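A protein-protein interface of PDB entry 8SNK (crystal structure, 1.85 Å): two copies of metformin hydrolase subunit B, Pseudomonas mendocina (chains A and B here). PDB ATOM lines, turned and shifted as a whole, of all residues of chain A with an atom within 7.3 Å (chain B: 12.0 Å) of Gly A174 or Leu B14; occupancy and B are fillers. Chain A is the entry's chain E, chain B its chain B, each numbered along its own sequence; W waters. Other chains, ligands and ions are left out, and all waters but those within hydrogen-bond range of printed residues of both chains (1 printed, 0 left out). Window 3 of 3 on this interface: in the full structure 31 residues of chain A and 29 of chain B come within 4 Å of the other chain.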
ATOM      1  N   SER A 171     -23.583  -1.462 -10.379  1.00  0.00           N
ATOM      2  CA  SER A 171     -24.858  -2.163 -10.315  1.00  0.00           C
ATOM      3  C   SER A 171     -24.696  -3.616 -10.755  1.00  0.00           C
ATOM      4  O   SER A 171     -23.711  -3.957 -11.429  1.00  0.00           O
ATOM      5  CB  SER A 171     -25.927  -1.467 -11.138  1.00  0.00           C
ATOM      6  OG  SER A 171     -25.630  -1.539 -12.516  1.00  0.00           O
ATOM      7  N   TRP A 172     -25.691  -4.425 -10.355  1.00  0.00           N
ATOM      8  CA  TRP A 172     -25.782  -5.846 -10.647  1.00  0.00           C
ATOM      9  C   TRP A 172     -27.205  -6.195 -11.082  1.00  0.00           C
ATOM     10  O   TRP A 172     -28.153  -6.032 -10.328  1.00  0.00           O
ATOM     11  CB  TRP A 172     -25.384  -6.680  -9.413  1.00  0.00           C
ATOM     12  CG  TRP A 172     -25.336  -8.169  -9.614  1.00  0.00           C
ATOM     13  CD1 TRP A 172     -26.379  -9.044  -9.624  1.00  0.00           C
ATOM     14  CD2 TRP A 172     -24.150  -8.972  -9.803  1.00  0.00           C
ATOM     15  NE1 TRP A 172     -25.934 -10.324  -9.818  1.00  0.00           N
ATOM     16  CE2 TRP A 172     -24.573 -10.316  -9.931  1.00  0.00           C
ATOM     17  CE3 TRP A 172     -22.783  -8.684  -9.886  1.00  0.00           C
ATOM     18  CZ2 TRP A 172     -23.675 -11.373 -10.109  1.00  0.00           C
ATOM     19  CZ3 TRP A 172     -21.894  -9.723 -10.080  1.00  0.00           C
ATOM     20  CH2 TRP A 172     -22.338 -11.050 -10.183  1.00  0.00           C
ATOM     21  N   ALA A 173     -27.339  -6.779 -12.274  1.00  0.00           N
ATOM     22  CA  ALA A 173     -28.643  -7.207 -12.742  1.00  0.00           C
ATOM     23  C   ALA A 173     -29.646  -6.066 -12.577  1.00  0.00           C
ATOM     24  O   ALA A 173     -30.773  -6.296 -12.125  1.00  0.00           O
ATOM     25  CB  ALA A 173     -29.078  -8.424 -11.977  1.00  0.00           C
ATOM     26  N   GLY A 174     -29.192  -4.847 -12.915  1.00  0.00           N
ATOM     27  CA  GLY A 174     -30.044  -3.667 -12.930  1.00  0.00           C
ATOM     28  C   GLY A 174     -30.332  -3.052 -11.559  1.00  0.00           C
ATOM     29  O   GLY A 174     -31.050  -2.054 -11.504  1.00  0.00           O
ATOM     30  N   GLU A 175     -29.736  -3.589 -10.474  1.00  0.00           N
ATOM     31  CA  GLU A 175     -29.979  -3.124  -9.114  1.00  0.00           C
ATOM     32  C   GLU A 175     -28.701  -2.567  -8.470  1.00  0.00           C
ATOM     33  O   GLU A 175     -27.604  -2.703  -9.013  1.00  0.00           O
ATOM     34  CB  GLU A 175     -30.547  -4.267  -8.288  1.00  0.00           C
ATOM     35  CG  GLU A 175     -31.879  -4.754  -8.808  1.00  0.00           C
ATOM     36  CD  GLU A 175     -32.603  -5.592  -7.781  1.00  0.00           C
ATOM     37  OE1 GLU A 175     -32.821  -5.089  -6.660  1.00  0.00           O
ATOM     38  OE2 GLU A 175     -32.924  -6.755  -8.097  1.00  0.00           O
ATOM     39  N   ARG A 176     -28.860  -1.886  -7.324  1.00  0.00           N
ATOM     40  CA  ARG A 176     -27.768  -1.116  -6.754  1.00  0.00           C
ATOM     41  C   ARG A 176     -27.530  -1.433  -5.273  1.00  0.00           C
ATOM     42  O   ARG A 176     -26.609  -0.871  -4.712  1.00  0.00           O
ATOM     43  CB  ARG A 176     -28.012   0.385  -6.950  1.00  0.00           C
ATOM     44  CG  ARG A 176     -28.324   0.813  -8.374  1.00  0.00           C
ATOM     45  CD  ARG A 176     -28.282   2.327  -8.513  1.00  0.00           C
ATOM     46  NE  ARG A 176     -26.949   2.823  -8.863  1.00  0.00           N
ATOM     47  CZ  ARG A 176     -26.194   3.610  -8.097  1.00  0.00           C
ATOM     48  NH1 ARG A 176     -24.975   3.935  -8.496  1.00  0.00           N
ATOM     49  NH2 ARG A 176     -26.634   4.035  -6.921  1.00  0.00           N
ATOM     50  N   ASN A 177     -28.265  -2.369  -4.666  1.00  0.00           N
ATOM     51  CA  ASN A 177     -28.162  -2.652  -3.233  1.00  0.00           C
ATOM     52  C   ASN A 177     -28.217  -4.157  -2.937  1.00  0.00           C
ATOM     53  O   ASN A 177     -28.554  -4.595  -1.836  1.00  0.00           O
ATOM     54  CB  ASN A 177     -29.218  -1.854  -2.465  1.00  0.00           C
ATOM     55  CG  ASN A 177     -28.827  -0.394  -2.373  1.00  0.00           C
ATOM     56  OD1 ASN A 177     -27.903  -0.042  -1.637  1.00  0.00           O
ATOM     57  ND2 ASN A 177     -29.475   0.460  -3.152  1.00  0.00           N
ATOM     58  N   LEU A 178     -27.854  -4.978  -3.922  1.00  0.00           N
ATOM     59  CA  LEU A 178     -27.684  -6.408  -3.724  1.00  0.00           C
ATOM     60  C   LEU A 178     -26.269  -6.625  -3.172  1.00  0.00           C
ATOM     61  O   LEU A 178     -25.464  -5.708  -3.185  1.00  0.00           O
ATOM     62  CB  LEU A 178     -27.896  -7.132  -5.063  1.00  0.00           C
ATOM     63  CG  LEU A 178     -29.264  -6.939  -5.724  1.00  0.00           C
ATOM     64  CD1 LEU A 178     -29.234  -7.430  -7.158  1.00  0.00           C
ATOM     65  CD2 LEU A 178     -30.369  -7.653  -4.956  1.00  0.00           C
ATOM     66  N   SER B   6     -18.582 -10.500 -28.021  1.00  0.00           N
ATOM     67  CA  SER B   6     -18.903  -9.608 -26.873  1.00  0.00           C
ATOM     68  C   SER B   6     -18.172 -10.089 -25.618  1.00  0.00           C
ATOM     69  O   SER B   6     -17.733 -11.239 -25.512  1.00  0.00           O
ATOM     70  CB  SER B   6     -20.407  -9.454 -26.632  1.00  0.00           C
ATOM     71  OG  SER B   6     -20.917 -10.427 -25.729  1.00  0.00           O
ATOM     72  N   TYR B   7     -18.056  -9.160 -24.671  1.00  0.00           N
ATOM     73  CA  TYR B   7     -17.241  -9.344 -23.492  1.00  0.00           C
ATOM     74  C   TYR B   7     -18.119  -9.140 -22.267  1.00  0.00           C
ATOM     75  O   TYR B   7     -17.625  -8.779 -21.206  1.00  0.00           O
ATOM     76  CB  TYR B   7     -16.057  -8.375 -23.546  1.00  0.00           C
ATOM     77  CG  TYR B   7     -15.059  -8.662 -24.641  1.00  0.00           C
ATOM     78  CD1 TYR B   7     -14.984  -7.859 -25.767  1.00  0.00           C
ATOM     79  CD2 TYR B   7     -14.181  -9.733 -24.547  1.00  0.00           C
ATOM     80  CE1 TYR B   7     -14.072  -8.120 -26.778  1.00  0.00           C
ATOM     81  CE2 TYR B   7     -13.260 -10.007 -25.548  1.00  0.00           C
ATOM     82  CZ  TYR B   7     -13.206  -9.195 -26.667  1.00  0.00           C
ATOM     83  OH  TYR B   7     -12.297  -9.460 -27.667  1.00  0.00           O
ATOM     84  N   ALA B   8     -19.421  -9.395 -22.405  1.00  0.00           N
ATOM     85  CA  ALA B   8     -20.360  -9.125 -21.323  1.00  0.00           C
ATOM     86  C   ALA B   8     -20.048  -9.993 -20.108  1.00  0.00           C
ATOM     87  O   ALA B   8     -20.344  -9.603 -18.985  1.00  0.00           O
ATOM     88  CB  ALA B   8     -21.767  -9.387 -21.777  1.00  0.00           C
ATOM     89  N   HIS B   9     -19.506 -11.188 -20.366  1.00  0.00           N
ATOM     90  CA  HIS B   9     -19.191 -12.174 -19.342  1.00  0.00           C
ATOM     91  C   HIS B   9     -18.027 -11.726 -18.450  1.00  0.00           C
ATOM     92  O   HIS B   9     -17.848 -12.301 -17.382  1.00  0.00           O
ATOM     93  CB  HIS B   9     -18.885 -13.536 -19.984  1.00  0.00           C
ATOM     94  CG  HIS B   9     -17.715 -13.475 -20.897  1.00  0.00           C
ATOM     95  ND1 HIS B   9     -17.847 -12.952 -22.161  1.00  0.00           N
ATOM     96  CD2 HIS B   9     -16.433 -13.823 -20.779  1.00  0.00           C
ATOM     97  CE1 HIS B   9     -16.671 -12.964 -22.777  1.00  0.00           C
ATOM     98  NE2 HIS B   9     -15.795 -13.521 -21.961  1.00  0.00           N
ATOM     99  N   LEU B  10     -17.216 -10.747 -18.876  1.00  0.00           N
ATOM    100  CA  LEU B  10     -16.119 -10.236 -18.064  1.00  0.00           C
ATOM    101  C   LEU B  10     -16.646  -9.423 -16.892  1.00  0.00           C
ATOM    102  O   LEU B  10     -15.899  -9.168 -15.962  1.00  0.00           O
ATOM    103  CB  LEU B  10     -15.208  -9.334 -18.900  1.00  0.00           C
ATOM    104  CG  LEU B  10     -14.546  -9.987 -20.103  1.00  0.00           C
ATOM    105  CD1 LEU B  10     -13.544  -9.032 -20.725  1.00  0.00           C
ATOM    106  CD2 LEU B  10     -13.872 -11.290 -19.707  1.00  0.00           C
ATOM    107  N   PHE B  11     -17.894  -8.957 -16.980  1.00  0.00           N
ATOM    108  CA  PHE B  11     -18.368  -7.888 -16.114  1.00  0.00           C
ATOM    109  C   PHE B  11     -19.608  -8.318 -15.363  1.00  0.00           C
ATOM    110  O   PHE B  11     -20.258  -9.284 -15.753  1.00  0.00           O
ATOM    111  CB  PHE B  11     -18.716  -6.632 -16.913  1.00  0.00           C
ATOM    112  CG  PHE B  11     -17.577  -6.092 -17.722  1.00  0.00           C
ATOM    113  CD1 PHE B  11     -16.555  -5.387 -17.122  1.00  0.00           C
ATOM    114  CD2 PHE B  11     -17.537  -6.302 -19.086  1.00  0.00           C
ATOM    115  CE1 PHE B  11     -15.526  -4.867 -17.885  1.00  0.00           C
ATOM    116  CE2 PHE B  11     -16.475  -5.837 -19.835  1.00  0.00           C
ATOM    117  CZ  PHE B  11     -15.480  -5.110 -19.244  1.00  0.00           C
ATOM    118  N   SER B  12     -19.929  -7.570 -14.293  1.00  0.00           N
ATOM    119  CA  SER B  12     -21.177  -7.767 -13.578  1.00  0.00           C
ATOM    120  C   SER B  12     -22.314  -7.826 -14.596  1.00  0.00           C
ATOM    121  O   SER B  12     -22.358  -6.991 -15.507  1.00  0.00           O
ATOM    122  CB  SER B  12     -21.464  -6.644 -12.585  1.00  0.00           C
ATOM    123  OG  SER B  12     -20.353  -6.303 -11.755  1.00  0.00           O
ATOM    124  N   PRO B  13     -23.318  -8.713 -14.422  1.00  0.00           N
ATOM    125  CA  PRO B  13     -24.373  -8.882 -15.425  1.00  0.00           C
ATOM    126  C   PRO B  13     -25.317  -7.688 -15.544  1.00  0.00           C
ATOM    127  O   PRO B  13     -25.229  -6.741 -14.752  1.00  0.00           O
ATOM    128  CB  PRO B  13     -25.155 -10.111 -14.938  1.00  0.00           C
ATOM    129  CG  PRO B  13     -24.877 -10.170 -13.443  1.00  0.00           C
ATOM    130  CD  PRO B  13     -23.491  -9.595 -13.260  1.00  0.00           C
ATOM    131  N   LEU B  14     -26.184  -7.755 -16.571  1.00  0.00           N
ATOM    132  CA  LEU B  14     -27.325  -6.864 -16.745  1.00  0.00           C
ATOM    133  C   LEU B  14     -28.597  -7.675 -16.480  1.00  0.00           C
ATOM    134  O   LEU B  14     -29.597  -7.040 -16.133  1.00  0.00           O
ATOM    135  CB  LEU B  14     -27.326  -6.297 -18.168  1.00  0.00           C
ATOM    136  CG  LEU B  14     -25.991  -5.750 -18.678  1.00  0.00           C
ATOM    137  CD1 LEU B  14     -26.043  -5.465 -20.164  1.00  0.00           C
ATOM    138  CD2 LEU B  14     -25.586  -4.483 -17.939  1.00  0.00           C
ATOM    139  N   PHE B  82     -17.332 -17.713 -12.551  1.00  0.00           N
ATOM    140  CA  PHE B  82     -17.149 -16.732 -13.610  1.00  0.00           C
ATOM    141  C   PHE B  82     -15.893 -17.098 -14.393  1.00  0.00           C
ATOM    142  O   PHE B  82     -15.053 -17.821 -13.893  1.00  0.00           O
ATOM    143  CB  PHE B  82     -17.072 -15.326 -13.026  1.00  0.00           C
ATOM    144  CG  PHE B  82     -18.339 -14.879 -12.338  1.00  0.00           C
ATOM    145  CD1 PHE B  82     -19.536 -15.552 -12.543  1.00  0.00           C
ATOM    146  CD2 PHE B  82     -18.339 -13.808 -11.462  1.00  0.00           C
ATOM    147  CE1 PHE B  82     -20.699 -15.149 -11.907  1.00  0.00           C
ATOM    148  CE2 PHE B  82     -19.496 -13.421 -10.802  1.00  0.00           C
ATOM    149  CZ  PHE B  82     -20.676 -14.077 -11.046  1.00  0.00           C
ATOM    150  N   ARG B 340     -13.845  -1.556 -20.733  1.00  0.00           N
ATOM    151  CA  ARG B 340     -14.727  -1.228 -19.616  1.00  0.00           C
ATOM    152  C   ARG B 340     -16.136  -1.750 -19.866  1.00  0.00           C
ATOM    153  O   ARG B 340     -16.505  -2.054 -20.991  1.00  0.00           O
ATOM    154  CB  ARG B 340     -14.800   0.282 -19.349  1.00  0.00           C
ATOM    155  CG  ARG B 340     -13.494   0.913 -18.896  1.00  0.00           C
ATOM    156  CD  ARG B 340     -13.140   0.534 -17.469  1.00  0.00           C
ATOM    157  NE  ARG B 340     -11.967   1.276 -17.034  1.00  0.00           N
ATOM    158  CZ  ARG B 340     -10.714   1.062 -17.440  1.00  0.00           C
ATOM    159  NH1 ARG B 340     -10.401   0.002 -18.167  1.00  0.00           N
ATOM    160  NH2 ARG B 340      -9.752   1.891 -17.071  1.00  0.00           N
ATOM    161  N   ARG B 341     -16.908  -1.860 -18.783  1.00  0.00           N
ATOM    162  CA  ARG B 341     -18.275  -2.333 -18.840  1.00  0.00           C
ATOM    163  C   ARG B 341     -19.159  -1.251 -19.455  1.00  0.00           C
ATOM    164  O   ARG B 341     -18.731  -0.103 -19.561  1.00  0.00           O
ATOM    165  CB  ARG B 341     -18.774  -2.613 -17.424  1.00  0.00           C
ATOM    166  CG  ARG B 341     -20.128  -3.298 -17.348  1.00  0.00           C
ATOM    167  CD  ARG B 341     -20.668  -3.234 -15.944  1.00  0.00           C
ATOM    168  NE  ARG B 341     -21.832  -4.075 -15.736  1.00  0.00           N
ATOM    169  CZ  ARG B 341     -23.023  -3.637 -15.339  1.00  0.00           C
ATOM    170  NH1 ARG B 341     -23.264  -2.339 -15.277  1.00  0.00           N
ATOM    171  NH2 ARG B 341     -23.972  -4.495 -15.014  1.00  0.00           N
ATOM    172  N   THR B 342     -20.394  -1.633 -19.819  1.00  0.00           N
ATOM    173  CA  THR B 342     -21.412  -0.728 -20.340  1.00  0.00           C
ATOM    174  C   THR B 342     -20.916  -0.135 -21.665  1.00  0.00           C
ATOM    175  O   THR B 342     -21.249   1.003 -22.003  1.00  0.00           O
ATOM    176  CB  THR B 342     -21.850   0.327 -19.300  1.00  0.00           C
ATOM    177  OG1 THR B 342     -20.853   1.336 -19.140  1.00  0.00           O
ATOM    178  CG2 THR B 342     -22.151  -0.243 -17.930  1.00  0.00           C
ATOM    179  N   ASP B 343     -20.127  -0.929 -22.413  1.00  0.00           N
ATOM    180  CA  ASP B 343     -19.563  -0.513 -23.691  1.00  0.00           C
ATOM    181  C   ASP B 343     -20.631  -0.645 -24.785  1.00  0.00           C
ATOM    182  O   ASP B 343     -21.565  -1.451 -24.583  1.00  0.00           O
ATOM    183  CB  ASP B 343     -18.307  -1.315 -24.056  1.00  0.00           C
ATOM    184  CG  ASP B 343     -16.978  -0.636 -23.755  1.00  0.00           C
ATOM    185  OD1 ASP B 343     -16.974   0.376 -23.021  1.00  0.00           O
ATOM    186  OD2 ASP B 343     -15.946  -1.113 -24.281  1.00  0.00           O
HETATM  187  O   HOH W   1     -21.396  -2.725 -12.342  1.00  0.00           O
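Of chain A, only Ala A173 (3.5 Å) and Gly A174 (3.9 Å) come within 4 Å of Leu B14. Of the printed residues of chain A, Phe B82 touches Trp A172 (3.6 Å). Printed residues of chain A within 4 Å of Arg B341: Ser A171 (3.6 Å). The nearest residue of chain B that does not touch Gly A174 is Pro B13 (4.8 Å). The nearest printed residue of chain A that does not touch Ser B12 is Ala A173 (5.6 Å).
No position is printed for both chains. Of the 8 pairs that touch across the chains among the printed residues, none has its exchanged pair printed and touching as well.
Among the printed residues, pairs that only touch across the chains: Ser A171 with Ser B12, Ser A171 with Arg B341, Trp A172 with Ser B12, Trp A172 with Pro B13, Trp A172 with Phe B82, Ala A173 with Leu B14 and Gly A174 with Leu B14.
NH2 of Arg B341 lies within hydrogen-bond range of O of Pro B13 (2.6 Å). NE of Arg B341 is in hydrogen-bond range of O of Ser B12, at 3.0 Å.
Of the 14 printed residues of chain B, 5 touch a printed residue of chain A. Hydrophobic or aromatic side chains of chain A within 4 Å of the printed part of chain B: Trp A172. Along chain A the printed residues that touch a printed residue of chain B span positions 171 to 174. Among the printed residues, no Asp or Glu carboxylate lies within 4 Å of a Lys or Arg side-chain nitrogen of the other chain.
The backbone carbonyl oxygen (O) of Pro B13 lies within hydrogen-bond range of the backbone NH (N) of Ala A173, at 3.3 Å.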
